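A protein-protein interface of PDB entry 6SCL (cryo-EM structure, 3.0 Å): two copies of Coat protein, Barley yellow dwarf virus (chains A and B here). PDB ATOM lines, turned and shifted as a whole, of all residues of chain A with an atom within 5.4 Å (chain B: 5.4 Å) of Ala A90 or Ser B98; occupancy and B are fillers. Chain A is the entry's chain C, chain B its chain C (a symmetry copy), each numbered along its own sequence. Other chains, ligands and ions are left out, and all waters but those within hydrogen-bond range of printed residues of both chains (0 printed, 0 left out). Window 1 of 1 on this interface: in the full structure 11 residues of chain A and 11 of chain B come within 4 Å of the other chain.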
ATOM      1  N   PHE A  64     -14.230  11.622  30.383  1.00  0.00           N
ATOM      2  CA  PHE A  64     -15.351  10.876  30.932  1.00  0.00           C
ATOM      3  C   PHE A  64     -14.946  10.215  32.239  1.00  0.00           C
ATOM      4  O   PHE A  64     -13.849   9.665  32.352  1.00  0.00           O
ATOM      5  CB  PHE A  64     -15.833   9.811  29.951  1.00  0.00           C
ATOM      6  CG  PHE A  64     -16.458  10.371  28.718  1.00  0.00           C
ATOM      7  CD1 PHE A  64     -17.781  10.768  28.723  1.00  0.00           C
ATOM      8  CD2 PHE A  64     -15.724  10.515  27.557  1.00  0.00           C
ATOM      9  CE1 PHE A  64     -18.360  11.290  27.590  1.00  0.00           C
ATOM     10  CE2 PHE A  64     -16.303  11.037  26.425  1.00  0.00           C
ATOM     11  CZ  PHE A  64     -17.620  11.423  26.443  1.00  0.00           C
ATOM     12  N   CYS A  88     -19.936   3.193  30.479  1.00  0.00           N
ATOM     13  CA  CYS A  88     -20.097   4.619  30.200  1.00  0.00           C
ATOM     14  C   CYS A  88     -20.908   4.741  28.921  1.00  0.00           C
ATOM     15  O   CYS A  88     -20.344   4.718  27.818  1.00  0.00           O
ATOM     16  CB  CYS A  88     -18.750   5.323  30.068  1.00  0.00           C
ATOM     17  SG  CYS A  88     -18.809   7.090  29.780  1.00  0.00           S
ATOM     18  N   PRO A  89     -22.237   4.860  29.017  1.00  0.00           N
ATOM     19  CA  PRO A  89     -23.055   5.029  27.809  1.00  0.00           C
ATOM     20  C   PRO A  89     -22.864   6.367  27.125  1.00  0.00           C
ATOM     21  O   PRO A  89     -23.239   6.497  25.953  1.00  0.00           O
ATOM     22  CB  PRO A  89     -24.487   4.883  28.334  1.00  0.00           C
ATOM     23  CG  PRO A  89     -24.349   4.152  29.615  1.00  0.00           C
ATOM     24  CD  PRO A  89     -23.070   4.633  30.206  1.00  0.00           C
ATOM     25  N   ALA A  90     -22.288   7.355  27.813  1.00  0.00           N
ATOM     26  CA  ALA A  90     -21.952   8.624  27.188  1.00  0.00           C
ATOM     27  C   ALA A  90     -20.853   8.486  26.146  1.00  0.00           C
ATOM     28  O   ALA A  90     -20.745   9.342  25.266  1.00  0.00           O
ATOM     29  CB  ALA A  90     -21.536   9.635  28.250  1.00  0.00           C
ATOM     30  N   LEU A  91     -20.030   7.443  26.230  1.00  0.00           N
ATOM     31  CA  LEU A  91     -19.108   7.104  25.157  1.00  0.00           C
ATOM     32  C   LEU A  91     -19.659   6.024  24.240  1.00  0.00           C
ATOM     33  O   LEU A  91     -19.588   6.168  23.024  1.00  0.00           O
ATOM     34  CB  LEU A  91     -17.766   6.632  25.719  1.00  0.00           C
ATOM     35  CG  LEU A  91     -16.691   6.470  24.643  1.00  0.00           C
ATOM     36  CD1 LEU A  91     -16.223   7.827  24.151  1.00  0.00           C
ATOM     37  CD2 LEU A  91     -15.524   5.609  25.072  1.00  0.00           C
ATOM     38  N   SER A  92     -20.227   4.956  24.802  1.00  0.00           N
ATOM     39  CA  SER A  92     -20.680   3.825  23.999  1.00  0.00           C
ATOM     40  C   SER A  92     -21.892   4.185  23.147  1.00  0.00           C
ATOM     41  O   SER A  92     -21.824   4.167  21.913  1.00  0.00           O
ATOM     42  CB  SER A  92     -21.010   2.648  24.913  1.00  0.00           C
ATOM     43  OG  SER A  92     -21.539   1.561  24.180  1.00  0.00           O
ATOM     44  N   ASP A  93     -23.013   4.517  23.787  1.00  0.00           N
ATOM     45  CA  ASP A  93     -24.232   4.902  23.087  1.00  0.00           C
ATOM     46  C   ASP A  93     -24.366   6.409  22.988  1.00  0.00           C
ATOM     47  O   ASP A  93     -25.476   6.945  22.988  1.00  0.00           O
ATOM     48  CB  ASP A  93     -25.456   4.307  23.778  1.00  0.00           C
ATOM     49  CG  ASP A  93     -25.528   2.807  23.633  1.00  0.00           C
ATOM     50  OD1 ASP A  93     -24.998   2.283  22.632  1.00  0.00           O
ATOM     51  OD2 ASP A  93     -26.120   2.150  24.514  1.00  0.00           O
ATOM     52  N   GLY A  94     -23.243   7.097  22.894  1.00  0.00           N
ATOM     53  CA  GLY A  94     -23.179   8.524  23.075  1.00  0.00           C
ATOM     54  C   GLY A  94     -22.370   9.180  21.988  1.00  0.00           C
ATOM     55  O   GLY A  94     -22.734   9.133  20.811  1.00  0.00           O
ATOM     56  N   ILE A  95     -21.272   9.818  22.394  1.00  0.00           N
ATOM     57  CA  ILE A  95     -20.478  10.642  21.501  1.00  0.00           C
ATOM     58  C   ILE A  95     -19.785   9.831  20.399  1.00  0.00           C
ATOM     59  O   ILE A  95     -19.468  10.390  19.343  1.00  0.00           O
ATOM     60  CB  ILE A  95     -19.493  11.465  22.357  1.00  0.00           C
ATOM     61  CG1 ILE A  95     -19.048  12.714  21.612  1.00  0.00           C
ATOM     62  CG2 ILE A  95     -18.288  10.651  22.761  1.00  0.00           C
ATOM     63  CD1 ILE A  95     -20.189  13.675  21.339  1.00  0.00           C
ATOM     64  N   LEU A  96     -19.596   8.517  20.572  1.00  0.00           N
ATOM     65  CA  LEU A  96     -19.021   7.718  19.496  1.00  0.00           C
ATOM     66  C   LEU A  96     -20.008   7.454  18.373  1.00  0.00           C
ATOM     67  O   LEU A  96     -19.595   7.032  17.289  1.00  0.00           O
ATOM     68  CB  LEU A  96     -18.504   6.376  20.007  1.00  0.00           C
ATOM     69  CG  LEU A  96     -17.147   6.379  20.697  1.00  0.00           C
ATOM     70  CD1 LEU A  96     -16.785   4.977  21.097  1.00  0.00           C
ATOM     71  CD2 LEU A  96     -16.115   6.931  19.770  1.00  0.00           C
ATOM     72  N   GLY B  94     -26.921  10.020  23.275  1.00  0.00           N
ATOM     73  CA  GLY B  94     -25.565  10.305  23.666  1.00  0.00           C
ATOM     74  C   GLY B  94     -25.487  10.720  25.111  1.00  0.00           C
ATOM     75  O   GLY B  94     -25.807   9.943  26.012  1.00  0.00           O
ATOM     76  N   ILE B  95     -25.031  11.954  25.331  1.00  0.00           N
ATOM     77  CA  ILE B  95     -24.734  12.445  26.664  1.00  0.00           C
ATOM     78  C   ILE B  95     -25.985  12.585  27.541  1.00  0.00           C
ATOM     79  O   ILE B  95     -25.870  12.547  28.771  1.00  0.00           O
ATOM     80  CB  ILE B  95     -23.944  13.763  26.523  1.00  0.00           C
ATOM     81  CG1 ILE B  95     -23.127  14.036  27.778  1.00  0.00           C
ATOM     82  CG2 ILE B  95     -24.854  14.934  26.238  1.00  0.00           C
ATOM     83  CD1 ILE B  95     -22.057  12.990  28.022  1.00  0.00           C
ATOM     84  N   LEU B  96     -27.187  12.677  26.959  1.00  0.00           N
ATOM     85  CA  LEU B  96     -28.391  12.718  27.783  1.00  0.00           C
ATOM     86  C   LEU B  96     -28.747  11.362  28.364  1.00  0.00           C
ATOM     87  O   LEU B  96     -29.568  11.292  29.283  1.00  0.00           O
ATOM     88  CB  LEU B  96     -29.592  13.235  26.995  1.00  0.00           C
ATOM     89  CG  LEU B  96     -29.696  14.743  26.810  1.00  0.00           C
ATOM     90  CD1 LEU B  96     -30.951  15.069  26.051  1.00  0.00           C
ATOM     91  CD2 LEU B  96     -29.717  15.411  28.145  1.00  0.00           C
ATOM     92  N   LYS B  97     -28.166  10.286  27.845  1.00  0.00           N
ATOM     93  CA  LYS B  97     -28.297   8.984  28.480  1.00  0.00           C
ATOM     94  C   LYS B  97     -27.394   8.833  29.695  1.00  0.00           C
ATOM     95  O   LYS B  97     -27.522   7.840  30.416  1.00  0.00           O
ATOM     96  CB  LYS B  97     -27.988   7.877  27.475  1.00  0.00           C
ATOM     97  CG  LYS B  97     -28.914   7.854  26.280  1.00  0.00           C
ATOM     98  CD  LYS B  97     -30.323   7.477  26.679  1.00  0.00           C
ATOM     99  CE  LYS B  97     -31.214   7.357  25.460  1.00  0.00           C
ATOM    100  NZ  LYS B  97     -32.611   7.013  25.827  1.00  0.00           N
ATOM    101  N   SER B  98     -26.492   9.781  29.941  1.00  0.00           N
ATOM    102  CA  SER B  98     -25.561   9.676  31.053  1.00  0.00           C
ATOM    103  C   SER B  98     -25.734  10.787  32.076  1.00  0.00           C
ATOM    104  O   SER B  98     -24.833  11.006  32.890  1.00  0.00           O
ATOM    105  CB  SER B  98     -24.127   9.668  30.535  1.00  0.00           C
ATOM    106  OG  SER B  98     -23.799  10.921  29.977  1.00  0.00           O
ATOM    107  N   TYR B  99     -26.858  11.495  32.055  1.00  0.00           N
ATOM    108  CA  TYR B  99     -27.131  12.548  33.021  1.00  0.00           C
ATOM    109  C   TYR B  99     -28.629  12.598  33.277  1.00  0.00           C
ATOM    110  O   TYR B  99     -29.427  12.226  32.416  1.00  0.00           O
ATOM    111  CB  TYR B  99     -26.633  13.907  32.531  1.00  0.00           C
ATOM    112  CG  TYR B  99     -25.130  14.085  32.528  1.00  0.00           C
ATOM    113  CD1 TYR B  99     -24.461  14.470  33.673  1.00  0.00           C
ATOM    114  CD2 TYR B  99     -24.388  13.876  31.380  1.00  0.00           C
ATOM    115  CE1 TYR B  99     -23.108  14.651  33.683  1.00  0.00           C
ATOM    116  CE2 TYR B  99     -23.022  14.051  31.381  1.00  0.00           C
ATOM    117  CZ  TYR B  99     -22.391  14.438  32.538  1.00  0.00           C
ATOM    118  OH  TYR B  99     -21.033  14.616  32.558  1.00  0.00           O
ATOM    119  N   HIS B 100     -29.005  13.056  34.472  1.00  0.00           N
ATOM    120  CA  HIS B 100     -30.423  13.212  34.783  1.00  0.00           C
ATOM    121  C   HIS B 100     -30.974  14.526  34.253  1.00  0.00           C
ATOM    122  O   HIS B 100     -31.978  14.541  33.536  1.00  0.00           O
ATOM    123  CB  HIS B 100     -30.671  13.135  36.288  1.00  0.00           C
ATOM    124  CG  HIS B 100     -30.604  11.754  36.852  1.00  0.00           C
ATOM    125  ND1 HIS B 100     -29.452  11.221  37.384  1.00  0.00           N
ATOM    126  CD2 HIS B 100     -31.553  10.798  36.972  1.00  0.00           C
ATOM    127  CE1 HIS B 100     -29.694   9.995  37.809  1.00  0.00           C
ATOM    128  NE2 HIS B 100     -30.962   9.713  37.570  1.00  0.00           N
ATOM    129  N   THR B 198     -26.135  16.127  37.444  1.00  0.00           N
ATOM    130  CA  THR B 198     -26.379  14.801  38.089  1.00  0.00           C
ATOM    131  C   THR B 198     -26.096  13.641  37.128  1.00  0.00           C
ATOM    132  O   THR B 198     -26.831  13.492  36.142  1.00  0.00           O
ATOM    133  CB  THR B 198     -27.732  14.726  38.809  1.00  0.00           C
ATOM    134  OG1 THR B 198     -27.611  15.438  40.039  1.00  0.00           O
ATOM    135  CG2 THR B 198     -28.176  13.307  39.085  1.00  0.00           C
ATOM    136  N   ALA B 199     -25.094  12.819  37.451  1.00  0.00           N
ATOM    137  CA  ALA B 199     -24.700  11.673  36.601  1.00  0.00           C
ATOM    138  C   ALA B 199     -25.760  10.568  36.657  1.00  0.00           C
ATOM    139  O   ALA B 199     -26.482  10.491  37.656  1.00  0.00           O
ATOM    140  CB  ALA B 199     -23.351  11.165  37.041  1.00  0.00           C
ATOM    141  N   LYS B 200     -25.849   9.754  35.601  1.00  0.00           N
ATOM    142  CA  LYS B 200     -26.793   8.652  35.571  1.00  0.00           C
ATOM    143  C   LYS B 200     -26.152   7.413  34.954  1.00  0.00           C
ATOM    144  O   LYS B 200     -25.318   7.514  34.056  1.00  0.00           O
ATOM    145  CB  LYS B 200     -28.044   9.053  34.791  1.00  0.00           C
ATOM    146  CG  LYS B 200     -29.124   7.997  34.736  1.00  0.00           C
ATOM    147  CD  LYS B 200     -30.376   8.534  34.077  1.00  0.00           C
ATOM    148  CE  LYS B 200     -30.186   8.697  32.583  1.00  0.00           C
ATOM    149  NZ  LYS B 200     -31.444   9.129  31.916  1.00  0.00           N
ATOM    150  OXT LYS B 200     -26.421   6.277  35.354  1.00  0.00           O
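The backbone NH of Gly A94 lies within hydrogen-bond range of the backbone carbonyl oxygen of Pro A89 (3.1 Å). N of Ile A95 lies within hydrogen-bond range of O of Ala A90 (3.0 Å). The side-chain hydroxyl (OG) of Ser B98 is in hydrogen-bond range of the backbone carbonyl oxygen (O) of Ile B95 (2.9 Å). The backbone carbonyl oxygen (O) of Ser B98 is in hydrogen-bond range of the backbone NH (N) of Lys B200.
Ala A90 touches just these residues of chain B: Ile B95 (3.4 Å) and Ser B98 (3.1 Å). Ser B98 touches just one residue of chain A: Ala A90 (3.1 Å). Printed residues of chain A within 4 Å of Gly B94: Asp A93 (3.4 Å) and Gly A94 (3.0 Å). Of the printed residues of chain B, Asp A93 touches Gly B94. Of the printed residues of chain B, Gly A94 touches Gly B94. Of the printed residues of chain A, Ile B95 touches Ala A90. The nearest residue of chain A that does not touch Ser B98 is Pro A89 (4.9 Å).
Among the printed residues, pairs that only touch across the chains: Gly A94 with Gly B94 (3.0 Å), Ala A90 with Ser B98 (3.1 Å) and Ala A90 with Ile B95 (3.4 Å).
Hydrophobic or aromatic side chains of chain A within 4 Å of the printed part of chain B: Ala A90.
Gly B94 touches its own counterpart, Gly A94. 3 positions are printed for both chains. Of the 4 pairs that touch across the chains among the printed residues, 1 has its exchanged pair printed and touching as well.
The backbone carbonyl oxygen of Asp A93 sits at hydrogen-bond distance from the backbone NH of Gly B94, at 3.4 Å.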
